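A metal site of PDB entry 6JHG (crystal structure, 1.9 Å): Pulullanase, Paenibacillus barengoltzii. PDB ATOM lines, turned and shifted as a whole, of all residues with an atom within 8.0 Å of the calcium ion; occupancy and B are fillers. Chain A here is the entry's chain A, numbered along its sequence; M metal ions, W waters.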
ATOM      1  N   VAL A 122     -23.665  15.549  15.754  1.00  0.00           N
ATOM      2  CA  VAL A 122     -24.505  14.806  14.822  1.00  0.00           C
ATOM      3  C   VAL A 122     -24.093  13.335  14.802  1.00  0.00           C
ATOM      4  O   VAL A 122     -22.992  12.966  15.211  1.00  0.00           O
ATOM      5  CB  VAL A 122     -24.443  15.368  13.369  1.00  0.00           C
ATOM      6  CG1 VAL A 122     -24.953  16.824  13.303  1.00  0.00           C
ATOM      7  CG2 VAL A 122     -23.023  15.226  12.762  1.00  0.00           C
ATOM      8  N   GLY A 123     -25.008  12.501  14.319  1.00  0.00           N
ATOM      9  CA  GLY A 123     -24.706  11.108  14.039  1.00  0.00           C
ATOM     10  C   GLY A 123     -23.933  10.979  12.736  1.00  0.00           C
ATOM     11  O   GLY A 123     -23.539  11.967  12.115  1.00  0.00           O
ATOM     12  N   VAL A 124     -23.716   9.727  12.322  1.00  0.00           N
ATOM     13  CA  VAL A 124     -22.955   9.481  11.098  1.00  0.00           C
ATOM     14  C   VAL A 124     -23.646  10.162   9.923  1.00  0.00           C
ATOM     15  O   VAL A 124     -24.875  10.116   9.784  1.00  0.00           O
ATOM     16  CB  VAL A 124     -22.765   7.974  10.874  1.00  0.00           C
ATOM     17  CG1 VAL A 124     -24.088   7.253  10.639  1.00  0.00           C
ATOM     18  CG2 VAL A 124     -21.805   7.720   9.710  1.00  0.00           C
ATOM     19  N   ASN A 125     -22.860  10.867   9.106  1.00  0.00           N
ATOM     20  CA  ASN A 125     -23.311  11.551   7.893  1.00  0.00           C
ATOM     21  C   ASN A 125     -24.297  12.675   8.170  1.00  0.00           C
ATOM     22  O   ASN A 125     -25.023  13.112   7.267  1.00  0.00           O
ATOM     23  CB  ASN A 125     -23.895  10.566   6.881  1.00  0.00           C
ATOM     24  CG  ASN A 125     -22.813   9.879   6.047  1.00  0.00           C
ATOM     25  OD1 ASN A 125     -21.808  10.498   5.686  1.00  0.00           O
ATOM     26  ND2 ASN A 125     -22.998   8.585   5.782  1.00  0.00           N
ATOM     27  N   GLY A 126     -24.371  13.138   9.428  1.00  0.00           N
ATOM     28  CA  GLY A 126     -25.042  14.381   9.757  1.00  0.00           C
ATOM     29  C   GLY A 126     -26.535  14.460   9.462  1.00  0.00           C
ATOM     30  O   GLY A 126     -27.031  15.548   9.156  1.00  0.00           O
ATOM     31  N   TYR A 215     -15.462  21.743   8.995  1.00  0.00           N
ATOM     32  CA  TYR A 215     -16.878  21.604   9.317  1.00  0.00           C
ATOM     33  C   TYR A 215     -17.437  20.386   8.554  1.00  0.00           C
ATOM     34  O   TYR A 215     -16.785  19.830   7.671  1.00  0.00           O
ATOM     35  CB  TYR A 215     -17.646  22.891   8.955  1.00  0.00           C
ATOM     36  CG  TYR A 215     -17.463  23.207   7.492  1.00  0.00           C
ATOM     37  CD1 TYR A 215     -18.232  22.577   6.525  1.00  0.00           C
ATOM     38  CD2 TYR A 215     -16.464  24.082   7.058  1.00  0.00           C
ATOM     39  CE1 TYR A 215     -18.038  22.800   5.184  1.00  0.00           C
ATOM     40  CE2 TYR A 215     -16.272  24.327   5.716  1.00  0.00           C
ATOM     41  CZ  TYR A 215     -17.061  23.679   4.780  1.00  0.00           C
ATOM     42  OH  TYR A 215     -16.886  23.859   3.435  1.00  0.00           O
ATOM     43  N   ASP A 216     -18.671  20.007   8.869  1.00  0.00           N
ATOM     44  CA  ASP A 216     -19.252  18.769   8.333  1.00  0.00           C
ATOM     45  C   ASP A 216     -19.756  18.999   6.907  1.00  0.00           C
ATOM     46  O   ASP A 216     -20.710  19.758   6.696  1.00  0.00           O
ATOM     47  CB  ASP A 216     -20.380  18.275   9.227  1.00  0.00           C
ATOM     48  CG  ASP A 216     -20.937  16.924   8.780  1.00  0.00           C
ATOM     49  OD1 ASP A 216     -20.168  16.111   8.242  1.00  0.00           O
ATOM     50  OD2 ASP A 216     -22.139  16.679   8.984  1.00  0.00           O
ATOM     51  N   TYR A 217     -19.127  18.350   5.941  1.00  0.00           N
ATOM     52  CA  TYR A 217     -19.545  18.501   4.548  1.00  0.00           C
ATOM     53  C   TYR A 217     -20.278  17.248   4.085  1.00  0.00           C
ATOM     54  O   TYR A 217     -20.467  16.272   4.837  1.00  0.00           O
ATOM     55  CB  TYR A 217     -18.345  18.857   3.656  1.00  0.00           C
ATOM     56  CG  TYR A 217     -17.119  17.961   3.720  1.00  0.00           C
ATOM     57  CD1 TYR A 217     -17.072  16.753   3.021  1.00  0.00           C
ATOM     58  CD2 TYR A 217     -15.978  18.377   4.405  1.00  0.00           C
ATOM     59  CE1 TYR A 217     -15.930  15.953   3.035  1.00  0.00           C
ATOM     60  CE2 TYR A 217     -14.841  17.586   4.421  1.00  0.00           C
ATOM     61  CZ  TYR A 217     -14.817  16.376   3.730  1.00  0.00           C
ATOM     62  OH  TYR A 217     -13.673  15.586   3.753  1.00  0.00           O
ATOM     63  N   SER A 218     -20.736  17.276   2.834  1.00  0.00           N
ATOM     64  CA  SER A 218     -21.840  16.420   2.430  1.00  0.00           C
ATOM     65  C   SER A 218     -21.412  14.972   2.211  1.00  0.00           C
ATOM     66  O   SER A 218     -20.263  14.678   1.859  1.00  0.00           O
ATOM     67  CB  SER A 218     -22.501  16.948   1.151  1.00  0.00           C
ATOM     68  OG  SER A 218     -21.668  16.735   0.031  1.00  0.00           O
ATOM     69  N   GLN A 219     -22.392  14.073   2.412  1.00  0.00           N
ATOM     70  CA  GLN A 219     -22.205  12.653   2.152  1.00  0.00           C
ATOM     71  C   GLN A 219     -21.830  12.376   0.700  1.00  0.00           C
ATOM     72  O   GLN A 219     -21.034  11.477   0.426  1.00  0.00           O
ATOM     73  CB  GLN A 219     -23.488  11.914   2.534  1.00  0.00           C
ATOM     74  CG  GLN A 219     -23.396  10.404   2.402  1.00  0.00           C
ATOM     75  CD  GLN A 219     -24.634   9.698   2.925  1.00  0.00           C
ATOM     76  OE1 GLN A 219     -25.453  10.293   3.639  1.00  0.00           O
ATOM     77  NE2 GLN A 219     -24.766   8.416   2.577  1.00  0.00           N
ATOM     78  N   GLU A 220     -22.387  13.127  -0.257  1.00  0.00           N
ATOM     79  CA  GLU A 220     -22.034  12.951  -1.654  1.00  0.00           C
ATOM     80  C   GLU A 220     -20.572  13.283  -1.926  1.00  0.00           C
ATOM     81  O   GLU A 220     -20.032  12.881  -2.961  1.00  0.00           O
ATOM     82  CB  GLU A 220     -22.914  13.824  -2.549  1.00  0.00           C
ATOM     83  CG  GLU A 220     -24.407  13.533  -2.414  1.00  0.00           C
ATOM     84  CD  GLU A 220     -25.148  14.615  -1.616  1.00  0.00           C
ATOM     85  OE1 GLU A 220     -24.838  14.790  -0.418  1.00  0.00           O
ATOM     86  OE2 GLU A 220     -26.024  15.299  -2.202  1.00  0.00           O
ATOM     87  N   SER A 221     -19.909  14.028  -1.033  1.00  0.00           N
ATOM     88  CA  SER A 221     -18.497  14.364  -1.188  1.00  0.00           C
ATOM     89  C   SER A 221     -17.611  13.255  -0.624  1.00  0.00           C
ATOM     90  O   SER A 221     -16.748  12.711  -1.317  1.00  0.00           O
ATOM     91  CB  SER A 221     -18.191  15.688  -0.483  1.00  0.00           C
ATOM     92  OG  SER A 221     -18.946  16.736  -1.053  1.00  0.00           O
ATOM     93  N   VAL A 222     -17.806  12.934   0.655  1.00  0.00           N
ATOM     94  CA  VAL A 222     -17.203  11.772   1.288  1.00  0.00           C
ATOM     95  C   VAL A 222     -18.311  11.103   2.101  1.00  0.00           C
ATOM     96  O   VAL A 222     -18.953  11.759   2.922  1.00  0.00           O
ATOM     97  CB  VAL A 222     -16.013  12.132   2.201  1.00  0.00           C
ATOM     98  CG1 VAL A 222     -15.546  10.914   2.977  1.00  0.00           C
ATOM     99  CG2 VAL A 222     -14.854  12.728   1.370  1.00  0.00           C
ATOM    100  N   ASP A 223     -18.552   9.823   1.853  1.00  0.00           N
ATOM    101  CA  ASP A 223     -19.558   9.074   2.596  1.00  0.00           C
ATOM    102  C   ASP A 223     -18.911   8.530   3.864  1.00  0.00           C
ATOM    103  O   ASP A 223     -18.041   7.663   3.796  1.00  0.00           O
ATOM    104  CB  ASP A 223     -20.144   7.946   1.738  1.00  0.00           C
ATOM    105  CG  ASP A 223     -21.319   7.247   2.403  1.00  0.00           C
ATOM    106  OD1 ASP A 223     -21.358   7.123   3.656  1.00  0.00           O
ATOM    107  OD2 ASP A 223     -22.224   6.817   1.646  1.00  0.00           O
ATOM    108  N   GLU A 224     -19.356   9.027   5.028  1.00  0.00           N
ATOM    109  CA  GLU A 224     -18.744   8.660   6.297  1.00  0.00           C
ATOM    110  C   GLU A 224     -18.988   7.204   6.661  1.00  0.00           C
ATOM    111  O   GLU A 224     -18.353   6.712   7.606  1.00  0.00           O
ATOM    112  CB  GLU A 224     -19.231   9.566   7.434  1.00  0.00           C
ATOM    113  CG  GLU A 224     -18.903  11.043   7.244  1.00  0.00           C
ATOM    114  CD  GLU A 224     -19.480  11.944   8.313  1.00  0.00           C
ATOM    115  OE1 GLU A 224     -20.050  11.416   9.304  1.00  0.00           O
ATOM    116  OE2 GLU A 224     -19.385  13.181   8.166  1.00  0.00           O
ATOM    117  N   ASP A 237     -18.591  21.677   0.274  1.00  0.00           N
ATOM    118  CA  ASP A 237     -20.023  21.401   0.151  1.00  0.00           C
ATOM    119  C   ASP A 237     -20.642  21.321   1.543  1.00  0.00           C
ATOM    120  O   ASP A 237     -20.837  20.234   2.083  1.00  0.00           O
ATOM    121  CB  ASP A 237     -20.264  20.088  -0.609  1.00  0.00           C
ATOM    122  CG  ASP A 237     -19.451  19.983  -1.883  1.00  0.00           C
ATOM    123  OD1 ASP A 237     -19.773  20.734  -2.835  1.00  0.00           O
ATOM    124  OD2 ASP A 237     -18.496  19.162  -1.922  1.00  0.00           O
ATOM    125  N   GLN A 239     -22.756  21.059   4.931  1.00  0.00           N
ATOM    126  CA  GLN A 239     -23.996  20.425   5.392  1.00  0.00           C
ATOM    127  C   GLN A 239     -24.360  20.840   6.814  1.00  0.00           C
ATOM    128  O   GLN A 239     -25.459  21.341   7.031  1.00  0.00           O
ATOM    129  CB  GLN A 239     -23.878  18.887   5.283  1.00  0.00           C
ATOM    130  CG  GLN A 239     -25.238  18.179   5.386  1.00  0.00           C
ATOM    131  CD  GLN A 239     -25.105  16.695   5.554  1.00  0.00           C
ATOM    132  OE1 GLN A 239     -24.129  16.093   5.089  1.00  0.00           O
ATOM    133  NE2 GLN A 239     -26.072  16.084   6.231  1.00  0.00           N
ATOM    134  N   ASN A 240     -23.467  20.650   7.791  1.00  0.00           N
ATOM    135  CA  ASN A 240     -23.686  21.139   9.162  1.00  0.00           C
ATOM    136  C   ASN A 240     -22.554  22.095   9.541  1.00  0.00           C
ATOM    137  O   ASN A 240     -21.433  21.651   9.829  1.00  0.00           O
ATOM    138  CB  ASN A 240     -23.789  19.979  10.131  1.00  0.00           C
ATOM    139  CG  ASN A 240     -24.968  19.083   9.832  1.00  0.00           C
ATOM    140  OD1 ASN A 240     -26.114  19.535   9.875  1.00  0.00           O
ATOM    141  ND2 ASN A 240     -24.704  17.823   9.498  1.00  0.00           N
ATOM    142  N   VAL A 243     -20.524  21.722  13.328  1.00  0.00           N
ATOM    143  CA  VAL A 243     -20.019  20.452  13.836  1.00  0.00           C
ATOM    144  C   VAL A 243     -18.868  20.006  12.948  1.00  0.00           C
ATOM    145  O   VAL A 243     -18.816  20.371  11.765  1.00  0.00           O
ATOM    146  CB  VAL A 243     -21.156  19.403  13.914  1.00  0.00           C
ATOM    147  CG1 VAL A 243     -21.644  19.035  12.539  1.00  0.00           C
ATOM    148  CG2 VAL A 243     -20.731  18.150  14.652  1.00  0.00           C
ATOM    149  N   PRO A 244     -17.874  19.270  13.472  1.00  0.00           N
ATOM    150  CA  PRO A 244     -16.766  18.806  12.622  1.00  0.00           C
ATOM    151  C   PRO A 244     -17.193  17.783  11.568  1.00  0.00           C
ATOM    152  O   PRO A 244     -18.197  17.093  11.705  1.00  0.00           O
ATOM    153  CB  PRO A 244     -15.794  18.150  13.605  1.00  0.00           C
ATOM    154  CG  PRO A 244     -16.103  18.799  14.935  1.00  0.00           C
ATOM    155  CD  PRO A 244     -17.591  19.077  14.903  1.00  0.00           C
ATOM    156  N   GLU A 245     -16.347  17.667  10.540  1.00  0.00           N
ATOM    157  CA  GLU A 245     -16.516  16.635   9.525  1.00  0.00           C
ATOM    158  C   GLU A 245     -16.209  15.261  10.104  1.00  0.00           C
ATOM    159  O   GLU A 245     -15.188  15.071  10.784  1.00  0.00           O
ATOM    160  CB  GLU A 245     -15.613  16.945   8.323  1.00  0.00           C
ATOM    161  CG  GLU A 245     -15.280  15.762   7.404  1.00  0.00           C
ATOM    162  CD  GLU A 245     -16.504  15.088   6.810  1.00  0.00           C
ATOM    163  OE1 GLU A 245     -17.560  15.741   6.724  1.00  0.00           O
ATOM    164  OE2 GLU A 245     -16.387  13.898   6.403  1.00  0.00           O
ATOM    165  N   GLY A 246     -17.094  14.293   9.851  1.00  0.00           N
ATOM    166  CA  GLY A 246     -16.969  12.977  10.478  1.00  0.00           C
ATOM    167  C   GLY A 246     -15.830  12.135   9.919  1.00  0.00           C
ATOM    168  O   GLY A 246     -15.233  11.345  10.654  1.00  0.00           O
ATOM    169  N   SER A 247     -15.501  12.285   8.635  1.00  0.00           N
ATOM    170  CA  SER A 247     -14.476  11.397   8.083  1.00  0.00           C
ATOM    171  C   SER A 247     -13.089  11.688   8.654  1.00  0.00           C
ATOM    172  O   SER A 247     -12.185  10.869   8.460  1.00  0.00           O
ATOM    173  CB  SER A 247     -14.451  11.481   6.549  1.00  0.00           C
ATOM    174  OG  SER A 247     -13.966  12.747   6.097  1.00  0.00           O
ATOM    175  N   TYR A 248     -12.900  12.811   9.342  1.00  0.00           N
ATOM    176  CA  TYR A 248     -11.615  13.115   9.979  1.00  0.00           C
ATOM    177  C   TYR A 248     -11.533  12.574  11.404  1.00  0.00           C
ATOM    178  O   TYR A 248     -10.497  12.748  12.069  1.00  0.00           O
ATOM    179  CB  TYR A 248     -11.334  14.635   9.939  1.00  0.00           C
ATOM    180  CG  TYR A 248     -11.331  15.194   8.520  1.00  0.00           C
ATOM    181  CD1 TYR A 248     -10.927  14.415   7.444  1.00  0.00           C
ATOM    182  CD2 TYR A 248     -11.716  16.517   8.270  1.00  0.00           C
ATOM    183  CE1 TYR A 248     -10.907  14.921   6.136  1.00  0.00           C
ATOM    184  CE2 TYR A 248     -11.698  17.045   6.960  1.00  0.00           C
ATOM    185  CZ  TYR A 248     -11.298  16.236   5.905  1.00  0.00           C
ATOM    186  OH  TYR A 248     -11.292  16.729   4.622  1.00  0.00           O
ATOM    187  N   PRO A 252     -16.895   7.931  12.961  1.00  0.00           N
ATOM    188  CA  PRO A 252     -17.966   8.880  12.622  1.00  0.00           C
ATOM    189  C   PRO A 252     -19.292   8.538  13.251  1.00  0.00           C
ATOM    190  O   PRO A 252     -20.204   9.379  13.202  1.00  0.00           O
ATOM    191  CB  PRO A 252     -18.049   8.774  11.088  1.00  0.00           C
ATOM    192  CG  PRO A 252     -16.881   7.949  10.658  1.00  0.00           C
ATOM    193  CD  PRO A 252     -16.469   7.113  11.809  1.00  0.00           C
ATOM    194  N   ARG A 258     -15.565  12.973  17.108  1.00  0.00           N
ATOM    195  CA  ARG A 258     -15.006  13.974  16.210  1.00  0.00           C
ATOM    196  C   ARG A 258     -14.760  15.289  16.926  1.00  0.00           C
ATOM    197  O   ARG A 258     -13.845  16.038  16.554  1.00  0.00           O
ATOM    198  CB  ARG A 258     -15.924  14.189  14.990  1.00  0.00           C
ATOM    199  CG  ARG A 258     -17.278  14.761  15.337  1.00  0.00           C
ATOM    200  CD  ARG A 258     -18.141  14.916  14.096  1.00  0.00           C
ATOM    201  NE  ARG A 258     -18.735  13.654  13.677  1.00  0.00           N
ATOM    202  CZ  ARG A 258     -19.534  13.509  12.623  1.00  0.00           C
ATOM    203  NH1 ARG A 258     -19.812  14.563  11.874  1.00  0.00           N
ATOM    204  NH2 ARG A 258     -20.043  12.317  12.320  1.00  0.00           N
HETATM  205 CA    CA M   1     -19.717  14.778   6.410  1.00  0.00          CA
HETATM  206  O   HOH W   1     -18.345  13.730   4.567  1.00  0.00           O
HETATM  207  O   HOH W   2     -22.004  14.435   6.560  1.00  0.00           O
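The calcium ion is bound by O of Tyr 217, 2.3 Å away.
OD1 of Asp 216 binds the calcium ion (2.3 Å).
The calcium ion is bound by water W2, 2.3 Å away.
OE1 of Glu 245 is bound to the calcium ion, at 2.4 Å.
OE2 of Glu 224 is bound to the calcium ion.
Water W1 is bound to the calcium ion, 2.5 Å away.
Of the 26 residues printed, 4 come within 4 Å of the calcium ion.
The nearest printed residue that does not touch the calcium ion is Gly 246 (4.4 Å).
N of Asn 125 sits at hydrogen-bond distance from OE1 of Glu 224, 2.9 Å away.
The backbone carbonyl oxygen (O) of Asp 216 lies within hydrogen-bond range of the backbone NH (N) of Gln 239 (3.0 Å).
The guanidinium group (NH2) of Arg 258 lies within salt-bridge range of the side-chain carboxylate (OE1) of Glu 224, at 3.1 Å.
The side-chain carboxylate (OE2) of Glu 224 lies close to the backbone NH (N) of Gly 246 (3.1 Å).
The side-chain carboxylate (OD1) of Asp 216 sits close to the guanidinium group (NH1) of Arg 258, at 3.96 Å.
The side-chain carboxylate (OE2) of Glu 245 is in hydrogen-bond range of the side-chain hydroxyl (OG) of Ser 247 (2.7 Å).
The backbone carbonyl oxygen of Val 243 is in hydrogen-bond range of the backbone NH of Asp 216, at 2.9 Å.
The side-chain hydroxyl (OH) of Tyr 248 lies within hydrogen-bond range of the side-chain hydroxyl (OH) of Tyr 217 (2.8 Å).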
